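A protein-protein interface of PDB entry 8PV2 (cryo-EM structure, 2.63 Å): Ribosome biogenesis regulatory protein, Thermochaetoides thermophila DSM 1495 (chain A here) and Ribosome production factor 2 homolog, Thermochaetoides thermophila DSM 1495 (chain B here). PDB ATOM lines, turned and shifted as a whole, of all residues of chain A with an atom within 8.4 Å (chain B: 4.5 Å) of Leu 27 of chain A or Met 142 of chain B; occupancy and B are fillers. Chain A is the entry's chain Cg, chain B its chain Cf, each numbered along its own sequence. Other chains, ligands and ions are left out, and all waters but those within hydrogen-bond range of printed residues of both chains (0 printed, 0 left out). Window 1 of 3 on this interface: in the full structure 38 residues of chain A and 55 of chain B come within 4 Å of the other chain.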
ATOM      1  N   THR A  22      -4.674 -24.534  -4.637  1.00  0.00           N
ATOM      2  CA  THR A  22      -4.334 -24.667  -3.229  1.00  0.00           C
ATOM      3  C   THR A  22      -4.942 -23.504  -2.462  1.00  0.00           C
ATOM      4  O   THR A  22      -5.237 -22.451  -3.027  1.00  0.00           O
ATOM      5  CB  THR A  22      -2.819 -24.731  -3.014  1.00  0.00           C
ATOM      6  OG1 THR A  22      -2.209 -23.530  -3.492  1.00  0.00           O
ATOM      7  CG2 THR A  22      -2.230 -25.920  -3.748  1.00  0.00           C
ATOM      8  N   PHE A  23      -5.157 -23.704  -1.168  1.00  0.00           N
ATOM      9  CA  PHE A  23      -5.924 -22.741  -0.400  1.00  0.00           C
ATOM     10  C   PHE A  23      -5.231 -22.422   0.912  1.00  0.00           C
ATOM     11  O   PHE A  23      -4.450 -23.217   1.437  1.00  0.00           O
ATOM     12  CB  PHE A  23      -7.340 -23.248  -0.114  1.00  0.00           C
ATOM     13  CG  PHE A  23      -8.184 -23.393  -1.338  1.00  0.00           C
ATOM     14  CD1 PHE A  23      -8.828 -22.296  -1.875  1.00  0.00           C
ATOM     15  CD2 PHE A  23      -8.339 -24.622  -1.946  1.00  0.00           C
ATOM     16  CE1 PHE A  23      -9.607 -22.420  -3.000  1.00  0.00           C
ATOM     17  CE2 PHE A  23      -9.121 -24.751  -3.073  1.00  0.00           C
ATOM     18  CZ  PHE A  23      -9.757 -23.650  -3.598  1.00  0.00           C
ATOM     19  N   ASP A  24      -5.528 -21.227   1.425  1.00  0.00           N
ATOM     20  CA  ASP A  24      -5.169 -20.805   2.774  1.00  0.00           C
ATOM     21  C   ASP A  24      -6.380 -20.005   3.255  1.00  0.00           C
ATOM     22  O   ASP A  24      -6.507 -18.805   3.007  1.00  0.00           O
ATOM     23  CB  ASP A  24      -3.879 -19.991   2.790  1.00  0.00           C
ATOM     24  CG  ASP A  24      -3.625 -19.325   4.121  1.00  0.00           C
ATOM     25  OD1 ASP A  24      -3.031 -18.232   4.124  1.00  0.00           O
ATOM     26  OD2 ASP A  24      -3.995 -19.900   5.165  1.00  0.00           O
ATOM     27  N   LEU A  25      -7.302 -20.694   3.926  1.00  0.00           N
ATOM     28  CA  LEU A  25      -8.579 -20.077   4.259  1.00  0.00           C
ATOM     29  C   LEU A  25      -8.477 -19.134   5.447  1.00  0.00           C
ATOM     30  O   LEU A  25      -9.430 -18.398   5.717  1.00  0.00           O
ATOM     31  CB  LEU A  25      -9.624 -21.157   4.526  1.00  0.00           C
ATOM     32  CG  LEU A  25      -9.904 -22.101   3.358  1.00  0.00           C
ATOM     33  CD1 LEU A  25     -11.065 -23.009   3.693  1.00  0.00           C
ATOM     34  CD2 LEU A  25     -10.191 -21.321   2.090  1.00  0.00           C
ATOM     35  N   GLY A  26      -7.357 -19.144   6.167  1.00  0.00           N
ATOM     36  CA  GLY A  26      -7.149 -18.145   7.198  1.00  0.00           C
ATOM     37  C   GLY A  26      -6.990 -16.748   6.637  1.00  0.00           C
ATOM     38  O   GLY A  26      -7.457 -15.777   7.236  1.00  0.00           O
ATOM     39  N   LEU A  27      -6.330 -16.625   5.487  1.00  0.00           N
ATOM     40  CA  LEU A  27      -6.171 -15.350   4.804  1.00  0.00           C
ATOM     41  C   LEU A  27      -7.155 -15.176   3.658  1.00  0.00           C
ATOM     42  O   LEU A  27      -7.063 -14.180   2.932  1.00  0.00           O
ATOM     43  CB  LEU A  27      -4.743 -15.199   4.280  1.00  0.00           C
ATOM     44  CG  LEU A  27      -3.614 -15.168   5.305  1.00  0.00           C
ATOM     45  CD1 LEU A  27      -2.281 -15.075   4.601  1.00  0.00           C
ATOM     46  CD2 LEU A  27      -3.790 -14.010   6.260  1.00  0.00           C
ATOM     47  N   LEU A  28      -8.093 -16.115   3.495  1.00  0.00           N
ATOM     48  CA  LEU A  28      -9.036 -16.152   2.370  1.00  0.00           C
ATOM     49  C   LEU A  28      -8.300 -16.113   1.035  1.00  0.00           C
ATOM     50  O   LEU A  28      -8.649 -15.353   0.133  1.00  0.00           O
ATOM     51  CB  LEU A  28     -10.062 -15.021   2.456  1.00  0.00           C
ATOM     52  CG  LEU A  28     -10.779 -14.783   3.783  1.00  0.00           C
ATOM     53  CD1 LEU A  28     -11.485 -13.450   3.744  1.00  0.00           C
ATOM     54  CD2 LEU A  28     -11.767 -15.894   4.056  1.00  0.00           C
ATOM     55  N   LEU A  29      -7.267 -16.937   0.910  1.00  0.00           N
ATOM     56  CA  LEU A  29      -6.356 -16.896  -0.222  1.00  0.00           C
ATOM     57  C   LEU A  29      -6.475 -18.179  -1.031  1.00  0.00           C
ATOM     58  O   LEU A  29      -6.527 -19.272  -0.463  1.00  0.00           O
ATOM     59  CB  LEU A  29      -4.920 -16.703   0.264  1.00  0.00           C
ATOM     60  CG  LEU A  29      -3.789 -16.915  -0.732  1.00  0.00           C
ATOM     61  CD1 LEU A  29      -3.853 -15.864  -1.806  1.00  0.00           C
ATOM     62  CD2 LEU A  29      -2.456 -16.878  -0.021  1.00  0.00           C
ATOM     63  N   ALA A  30      -6.522 -18.040  -2.354  1.00  0.00           N
ATOM     64  CA  ALA A  30      -6.505 -19.167  -3.276  1.00  0.00           C
ATOM     65  C   ALA A  30      -5.346 -18.995  -4.243  1.00  0.00           C
ATOM     66  O   ALA A  30      -5.185 -17.926  -4.838  1.00  0.00           O
ATOM     67  CB  ALA A  30      -7.820 -19.278  -4.045  1.00  0.00           C
ATOM     68  N   ASN A  31      -4.545 -20.042  -4.401  1.00  0.00           N
ATOM     69  CA  ASN A  31      -3.404 -20.045  -5.305  1.00  0.00           C
ATOM     70  C   ASN A  31      -3.729 -20.955  -6.480  1.00  0.00           C
ATOM     71  O   ASN A  31      -4.022 -22.143  -6.293  1.00  0.00           O
ATOM     72  CB  ASN A  31      -2.139 -20.512  -4.594  1.00  0.00           C
ATOM     73  CG  ASN A  31      -1.724 -19.587  -3.480  1.00  0.00           C
ATOM     74  OD1 ASN A  31      -1.736 -19.962  -2.308  1.00  0.00           O
ATOM     75  ND2 ASN A  31      -1.361 -18.363  -3.835  1.00  0.00           N
ATOM     76  N   ASP A  32      -3.672 -20.389  -7.686  1.00  0.00           N
ATOM     77  CA  ASP A  32      -3.858 -21.135  -8.918  1.00  0.00           C
ATOM     78  C   ASP A  32      -2.526 -21.227  -9.642  1.00  0.00           C
ATOM     79  O   ASP A  32      -2.070 -20.221 -10.206  1.00  0.00           O
ATOM     80  CB  ASP A  32      -4.897 -20.461  -9.806  1.00  0.00           C
ATOM     81  CG  ASP A  32      -4.902 -21.010 -11.217  1.00  0.00           C
ATOM     82  OD1 ASP A  32      -4.666 -20.227 -12.161  1.00  0.00           O
ATOM     83  OD2 ASP A  32      -5.137 -22.225 -11.381  1.00  0.00           O
ATOM     84  N   GLY A  58     -11.405 -18.393  -9.911  1.00  0.00           N
ATOM     85  CA  GLY A  58     -10.799 -18.363  -8.587  1.00  0.00           C
ATOM     86  C   GLY A  58     -11.799 -18.068  -7.485  1.00  0.00           C
ATOM     87  O   GLY A  58     -11.780 -18.705  -6.426  1.00  0.00           O
ATOM     88  N   ALA A  59     -12.699 -17.112  -7.726  1.00  0.00           N
ATOM     89  CA  ALA A  59     -13.734 -16.798  -6.750  1.00  0.00           C
ATOM     90  C   ALA A  59     -14.678 -17.972  -6.546  1.00  0.00           C
ATOM     91  O   ALA A  59     -15.100 -18.246  -5.418  1.00  0.00           O
ATOM     92  CB  ALA A  59     -14.508 -15.559  -7.190  1.00  0.00           C
ATOM     93  N   LEU A  62     -12.917 -20.658  -4.474  1.00  0.00           N
ATOM     94  CA  LEU A  62     -12.765 -20.175  -3.105  1.00  0.00           C
ATOM     95  C   LEU A  62     -14.083 -20.244  -2.342  1.00  0.00           C
ATOM     96  O   LEU A  62     -14.117 -20.659  -1.176  1.00  0.00           O
ATOM     97  CB  LEU A  62     -12.222 -18.749  -3.126  1.00  0.00           C
ATOM     98  CG  LEU A  62     -11.614 -18.191  -1.846  1.00  0.00           C
ATOM     99  CD1 LEU A  62     -10.638 -19.174  -1.250  1.00  0.00           C
ATOM    100  CD2 LEU A  62     -10.910 -16.905  -2.188  1.00  0.00           C
ATOM    101  N   LEU A  66     -14.786 -22.614   0.934  1.00  0.00           N
ATOM    102  CA  LEU A  66     -15.256 -22.039   2.191  1.00  0.00           C
ATOM    103  C   LEU A  66     -16.596 -22.624   2.614  1.00  0.00           C
ATOM    104  O   LEU A  66     -16.815 -22.886   3.801  1.00  0.00           O
ATOM    105  CB  LEU A  66     -15.358 -20.521   2.071  1.00  0.00           C
ATOM    106  CG  LEU A  66     -14.052 -19.735   2.082  1.00  0.00           C
ATOM    107  CD1 LEU A  66     -14.275 -18.347   1.525  1.00  0.00           C
ATOM    108  CD2 LEU A  66     -13.516 -19.657   3.491  1.00  0.00           C
ATOM    109  N   LEU A  83     -12.810 -20.317  10.607  1.00  0.00           N
ATOM    110  CA  LEU A  83     -11.660 -20.395   9.720  1.00  0.00           C
ATOM    111  C   LEU A  83     -10.470 -21.031  10.423  1.00  0.00           C
ATOM    112  O   LEU A  83     -10.290 -20.846  11.630  1.00  0.00           O
ATOM    113  CB  LEU A  83     -11.258 -19.006   9.226  1.00  0.00           C
ATOM    114  CG  LEU A  83     -12.268 -18.221   8.396  1.00  0.00           C
ATOM    115  CD1 LEU A  83     -11.786 -16.799   8.221  1.00  0.00           C
ATOM    116  CD2 LEU A  83     -12.470 -18.884   7.057  1.00  0.00           C
ATOM    117  N   PRO A  84      -9.651 -21.784   9.687  1.00  0.00           N
ATOM    118  CA  PRO A  84      -8.412 -22.287  10.266  1.00  0.00           C
ATOM    119  C   PRO A  84      -7.418 -21.154  10.457  1.00  0.00           C
ATOM    120  O   PRO A  84      -7.554 -20.085   9.841  1.00  0.00           O
ATOM    121  CB  PRO A  84      -7.916 -23.297   9.216  1.00  0.00           C
ATOM    122  CG  PRO A  84      -8.512 -22.821   7.948  1.00  0.00           C
ATOM    123  CD  PRO A  84      -9.853 -22.272   8.312  1.00  0.00           C
ATOM    124  N   PRO A  85      -6.426 -21.330  11.326  1.00  0.00           N
ATOM    125  CA  PRO A  85      -5.359 -20.329  11.449  1.00  0.00           C
ATOM    126  C   PRO A  85      -4.562 -20.224  10.163  1.00  0.00           C
ATOM    127  O   PRO A  85      -4.453 -21.208   9.415  1.00  0.00           O
ATOM    128  CB  PRO A  85      -4.496 -20.870  12.600  1.00  0.00           C
ATOM    129  CG  PRO A  85      -4.851 -22.309  12.707  1.00  0.00           C
ATOM    130  CD  PRO A  85      -6.286 -22.402  12.324  1.00  0.00           C
ATOM    131  N   PRO A  86      -4.024 -19.042   9.852  1.00  0.00           N
ATOM    132  CA  PRO A  86      -3.303 -18.865   8.585  1.00  0.00           C
ATOM    133  C   PRO A  86      -2.034 -19.700   8.529  1.00  0.00           C
ATOM    134  O   PRO A  86      -1.321 -19.852   9.523  1.00  0.00           O
ATOM    135  CB  PRO A  86      -2.987 -17.366   8.566  1.00  0.00           C
ATOM    136  CG  PRO A  86      -3.954 -16.757   9.514  1.00  0.00           C
ATOM    137  CD  PRO A  86      -4.154 -17.775  10.586  1.00  0.00           C
ATOM    138  N   THR A  87      -1.756 -20.242   7.345  1.00  0.00           N
ATOM    139  CA  THR A  87      -0.589 -21.083   7.126  1.00  0.00           C
ATOM    140  C   THR A  87       0.440 -20.465   6.196  1.00  0.00           C
ATOM    141  O   THR A  87       1.554 -20.981   6.104  1.00  0.00           O
ATOM    142  CB  THR A  87      -1.008 -22.442   6.556  1.00  0.00           C
ATOM    143  OG1 THR A  87      -1.676 -22.250   5.304  1.00  0.00           O
ATOM    144  CG2 THR A  87      -1.941 -23.156   7.515  1.00  0.00           C
ATOM    145  N   THR A  88       0.096 -19.388   5.506  1.00  0.00           N
ATOM    146  CA  THR A  88       1.045 -18.717   4.634  1.00  0.00           C
ATOM    147  C   THR A  88       2.095 -18.005   5.477  1.00  0.00           C
ATOM    148  O   THR A  88       1.736 -17.176   6.327  1.00  0.00           O
ATOM    149  CB  THR A  88       0.332 -17.719   3.727  1.00  0.00           C
ATOM    150  OG1 THR A  88      -0.553 -18.422   2.848  1.00  0.00           O
ATOM    151  CG2 THR A  88       1.337 -16.943   2.901  1.00  0.00           C
ATOM    152  N   PRO A  89       3.381 -18.297   5.292  1.00  0.00           N
ATOM    153  CA  PRO A  89       4.409 -17.663   6.124  1.00  0.00           C
ATOM    154  C   PRO A  89       4.602 -16.204   5.740  1.00  0.00           C
ATOM    155  O   PRO A  89       4.925 -15.886   4.594  1.00  0.00           O
ATOM    156  CB  PRO A  89       5.663 -18.495   5.829  1.00  0.00           C
ATOM    157  CG  PRO A  89       5.170 -19.735   5.153  1.00  0.00           C
ATOM    158  CD  PRO A  89       3.950 -19.324   4.411  1.00  0.00           C
ATOM    159  N   LEU A  90       4.406 -15.318   6.711  1.00  0.00           N
ATOM    160  CA  LEU A  90       4.539 -13.885   6.514  1.00  0.00           C
ATOM    161  C   LEU A  90       5.438 -13.319   7.601  1.00  0.00           C
ATOM    162  O   LEU A  90       5.394 -13.782   8.747  1.00  0.00           O
ATOM    163  CB  LEU A  90       3.169 -13.189   6.543  1.00  0.00           C
ATOM    164  CG  LEU A  90       2.278 -13.478   5.335  1.00  0.00           C
ATOM    165  CD1 LEU A  90       0.832 -13.162   5.641  1.00  0.00           C
ATOM    166  CD2 LEU A  90       2.746 -12.683   4.139  1.00  0.00           C
ATOM    167  N   PRO B 140     -11.022  -8.029   1.550  1.00  0.00           N
ATOM    168  CA  PRO B 140     -11.337  -8.817   0.361  1.00  0.00           C
ATOM    169  C   PRO B 140     -10.611 -10.154   0.386  1.00  0.00           C
ATOM    170  O   PRO B 140      -9.565 -10.316   1.016  1.00  0.00           O
ATOM    171  CB  PRO B 140     -10.815  -7.932  -0.775  1.00  0.00           C
ATOM    172  CG  PRO B 140      -9.637  -7.256  -0.172  1.00  0.00           C
ATOM    173  CD  PRO B 140      -9.933  -7.071   1.297  1.00  0.00           C
ATOM    174  N   MET B 141     -11.188 -11.122  -0.311  1.00  0.00           N
ATOM    175  CA  MET B 141     -10.446 -12.355  -0.509  1.00  0.00           C
ATOM    176  C   MET B 141      -9.403 -12.149  -1.598  1.00  0.00           C
ATOM    177  O   MET B 141      -9.455 -11.186  -2.358  1.00  0.00           O
ATOM    178  CB  MET B 141     -11.373 -13.516  -0.852  1.00  0.00           C
ATOM    179  CG  MET B 141     -12.691 -13.480  -0.120  1.00  0.00           C
ATOM    180  SD  MET B 141     -13.773 -14.826  -0.607  1.00  0.00           S
ATOM    181  CE  MET B 141     -14.648 -14.063  -1.953  1.00  0.00           C
ATOM    182  N   MET B 142      -8.431 -13.050  -1.649  1.00  0.00           N
ATOM    183  CA  MET B 142      -7.292 -12.882  -2.535  1.00  0.00           C
ATOM    184  C   MET B 142      -7.115 -14.106  -3.415  1.00  0.00           C
ATOM    185  O   MET B 142      -7.249 -15.242  -2.953  1.00  0.00           O
ATOM    186  CB  MET B 142      -6.015 -12.619  -1.741  1.00  0.00           C
ATOM    187  CG  MET B 142      -5.957 -11.242  -1.110  1.00  0.00           C
ATOM    188  SD  MET B 142      -4.483 -10.984  -0.117  1.00  0.00           S
ATOM    189  CE  MET B 142      -4.786 -12.115   1.230  1.00  0.00           C
ATOM    190  N   VAL B 143      -6.825 -13.863  -4.689  1.00  0.00           N
ATOM    191  CA  VAL B 143      -6.508 -14.907  -5.654  1.00  0.00           C
ATOM    192  C   VAL B 143      -5.204 -14.512  -6.329  1.00  0.00           C
ATOM    193  O   VAL B 143      -5.081 -13.390  -6.832  1.00  0.00           O
ATOM    194  CB  VAL B 143      -7.627 -15.093  -6.693  1.00  0.00           C
ATOM    195  CG1 VAL B 143      -7.183 -16.018  -7.806  1.00  0.00           C
ATOM    196  CG2 VAL B 143      -8.880 -15.628  -6.037  1.00  0.00           C
ATOM    197  N   PHE B 144      -4.228 -15.413  -6.315  1.00  0.00           N
ATOM    198  CA  PHE B 144      -2.954 -15.213  -6.997  1.00  0.00           C
ATOM    199  C   PHE B 144      -2.832 -16.282  -8.071  1.00  0.00           C
ATOM    200  O   PHE B 144      -2.729 -17.471  -7.761  1.00  0.00           O
ATOM    201  CB  PHE B 144      -1.787 -15.272  -6.018  1.00  0.00           C
ATOM    202  CG  PHE B 144      -1.572 -13.995  -5.269  1.00  0.00           C
ATOM    203  CD1 PHE B 144      -2.368 -13.674  -4.187  1.00  0.00           C
ATOM    204  CD2 PHE B 144      -0.592 -13.106  -5.659  1.00  0.00           C
ATOM    205  CE1 PHE B 144      -2.183 -12.497  -3.499  1.00  0.00           C
ATOM    206  CE2 PHE B 144      -0.402 -11.926  -4.977  1.00  0.00           C
ATOM    207  CZ  PHE B 144      -1.199 -11.622  -3.894  1.00  0.00           C
ATOM    208  N   LEU B 164       2.026  -8.221  -1.415  1.00  0.00           N
ATOM    209  CA  LEU B 164       0.622  -7.944  -1.698  1.00  0.00           C
ATOM    210  C   LEU B 164      -0.304  -8.672  -0.731  1.00  0.00           C
ATOM    211  O   LEU B 164      -1.341  -8.121  -0.341  1.00  0.00           O
ATOM    212  CB  LEU B 164       0.294  -8.303  -3.145  1.00  0.00           C
ATOM    213  CG  LEU B 164       0.914  -7.403  -4.214  1.00  0.00           C
ATOM    214  CD1 LEU B 164       0.606  -7.934  -5.595  1.00  0.00           C
ATOM    215  CD2 LEU B 164       0.444  -5.973  -4.075  1.00  0.00           C
ATOM    216  N   ILE B 165       0.053  -9.895  -0.325  1.00  0.00           N
ATOM    217  CA  ILE B 165      -0.702 -10.586   0.717  1.00  0.00           C
ATOM    218  C   ILE B 165      -0.619  -9.820   2.030  1.00  0.00           C
ATOM    219  O   ILE B 165      -1.631  -9.610   2.709  1.00  0.00           O
ATOM    220  CB  ILE B 165      -0.196 -12.031   0.875  1.00  0.00           C
ATOM    221  CG1 ILE B 165      -0.600 -12.870  -0.329  1.00  0.00           C
ATOM    222  CG2 ILE B 165      -0.752 -12.667   2.131  1.00  0.00           C
ATOM    223  CD1 ILE B 165       0.106 -14.193  -0.394  1.00  0.00           C
ATOM    224  N   PHE B 168      -2.949  -6.682   1.675  1.00  0.00           N
ATOM    225  CA  PHE B 168      -4.391  -6.877   1.617  1.00  0.00           C
ATOM    226  C   PHE B 168      -4.922  -7.839   2.675  1.00  0.00           C
ATOM    227  O   PHE B 168      -6.110  -8.164   2.644  1.00  0.00           O
ATOM    228  CB  PHE B 168      -4.808  -7.385   0.235  1.00  0.00           C
ATOM    229  CG  PHE B 168      -4.688  -6.368  -0.858  1.00  0.00           C
ATOM    230  CD1 PHE B 168      -5.552  -5.288  -0.920  1.00  0.00           C
ATOM    231  CD2 PHE B 168      -3.731  -6.508  -1.848  1.00  0.00           C
ATOM    232  CE1 PHE B 168      -5.448  -4.356  -1.939  1.00  0.00           C
ATOM    233  CE2 PHE B 168      -3.623  -5.580  -2.866  1.00  0.00           C
ATOM    234  CZ  PHE B 168      -4.484  -4.506  -2.913  1.00  0.00           C
ATOM    235  N   ARG B 169      -4.081  -8.310   3.601  1.00  0.00           N
ATOM    236  CA  ARG B 169      -4.529  -9.345   4.530  1.00  0.00           C
ATOM    237  C   ARG B 169      -5.535  -8.809   5.544  1.00  0.00           C
ATOM    238  O   ARG B 169      -6.383  -9.563   6.033  1.00  0.00           O
ATOM    239  CB  ARG B 169      -3.339  -9.974   5.255  1.00  0.00           C
ATOM    240  CG  ARG B 169      -2.562  -9.012   6.117  1.00  0.00           C
ATOM    241  CD  ARG B 169      -1.403  -9.678   6.809  1.00  0.00           C
ATOM    242  NE  ARG B 169      -1.853 -10.710   7.732  1.00  0.00           N
ATOM    243  CZ  ARG B 169      -1.041 -11.474   8.447  1.00  0.00           C
ATOM    244  NH1 ARG B 169       0.271 -11.310   8.408  1.00  0.00           N
ATOM    245  NH2 ARG B 169      -1.558 -12.412   9.234  1.00  0.00           N
ATOM    246  N   VAL B 185      -9.658  -9.686  -4.774  1.00  0.00           N
ATOM    247  CA  VAL B 185      -8.506  -9.061  -5.405  1.00  0.00           C
ATOM    248  C   VAL B 185      -7.720 -10.152  -6.109  1.00  0.00           C
ATOM    249  O   VAL B 185      -7.283 -11.117  -5.475  1.00  0.00           O
ATOM    250  CB  VAL B 185      -7.630  -8.340  -4.370  1.00  0.00           C
ATOM    251  CG1 VAL B 185      -6.364  -7.856  -5.011  1.00  0.00           C
ATOM    252  CG2 VAL B 185      -8.384  -7.187  -3.748  1.00  0.00           C
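Leu 27 of chain A touches Met 142 of chain B (O to CE, 3.5 Å). Ile 165 of chain B touches Leu 27 of chain A. Met 141 of chain B touches Leu 28 of chain A. CA of Leu 29 of chain A touches O of Met 142 of chain B (3.3 Å). CD1 of Leu 29 of chain A touches CD1 of Phe 144 of chain B, 3.6 Å away. Ile 165 of chain B touches Leu 29 of chain A (CD1 to CD2, 3.7 Å). Ala 30 of chain A touches Val 143 of chain B. Phe 144 of chain B touches Asn 31 of chain A. Met 141 of chain B touches Leu 62 of chain A. Ile 165 of chain B touches Leu 90 of chain A.
The backbone carbonyl oxygen (O) of Ala 30 of chain A lies within hydrogen-bond range of the backbone NH (N) of Phe 144 of chain B (3.1 Å). The backbone carbonyl oxygen (O) of Leu 28 of chain A is in hydrogen-bond range of the backbone NH (N) of Met 142 of chain B (2.9 Å). The backbone carbonyl oxygen (O) of Met 142 of chain B sits at hydrogen-bond distance from the backbone NH (N) of Ala 30 of chain A, 3.0 Å away. N of Asp 32 of chain A lies within hydrogen-bond range of O of Phe 144 of chain B, at 3.1 Å.
The backbone NH (N) of Val 185 of chain B lies within hydrogen-bond range of the backbone carbonyl oxygen (O) of Met 141 of chain B, 2.9 Å away. The backbone carbonyl oxygen (O) of Thr 22 of chain A sits at hydrogen-bond distance from the backbone NH (N) of Asn 31 of chain A, 2.9 Å away. The backbone carbonyl oxygen of Val 185 of chain B sits at hydrogen-bond distance from the backbone NH of Val 143 of chain B (2.9 Å). The backbone NH (N) of Asp 24 of chain A is in hydrogen-bond range of the backbone carbonyl oxygen (O) of Leu 29 of chain A.
Leu 27 of chain A touches just these residues of chain B: Met 142 and Ile 165. Pro 89 of chain A touches none of the printed residues of chain B. Leu 164 of chain B touches none of the printed residues of chain A. Of the printed residues of chain A, Ile 165 of chain B touches Leu 27, Leu 29 and Leu 90. Printed residues of chain A within 4 Å of Arg 169 of chain B: Leu 90. The nearest residue of chain A that does not touch Met 142 of chain B is Leu 62 of chain A (4.1 Å). The nearest printed residue of chain A that does not touch Arg 169 of chain B is Leu 27 of chain A (4.05 Å).
Hydrophobic or aromatic side chains of chain A within 4 Å of the printed part of chain B: Leu 27, Leu 28, Leu 29, Leu 62 and Leu 90. Of the 10 printed residues of chain B, 6 touch a printed residue of chain A. Among the printed residues, 15 pairs touch across the chains. Among the printed residues, no Asp or Glu carboxylate lies within 4 Å of a Lys or Arg side-chain nitrogen of the other chain.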
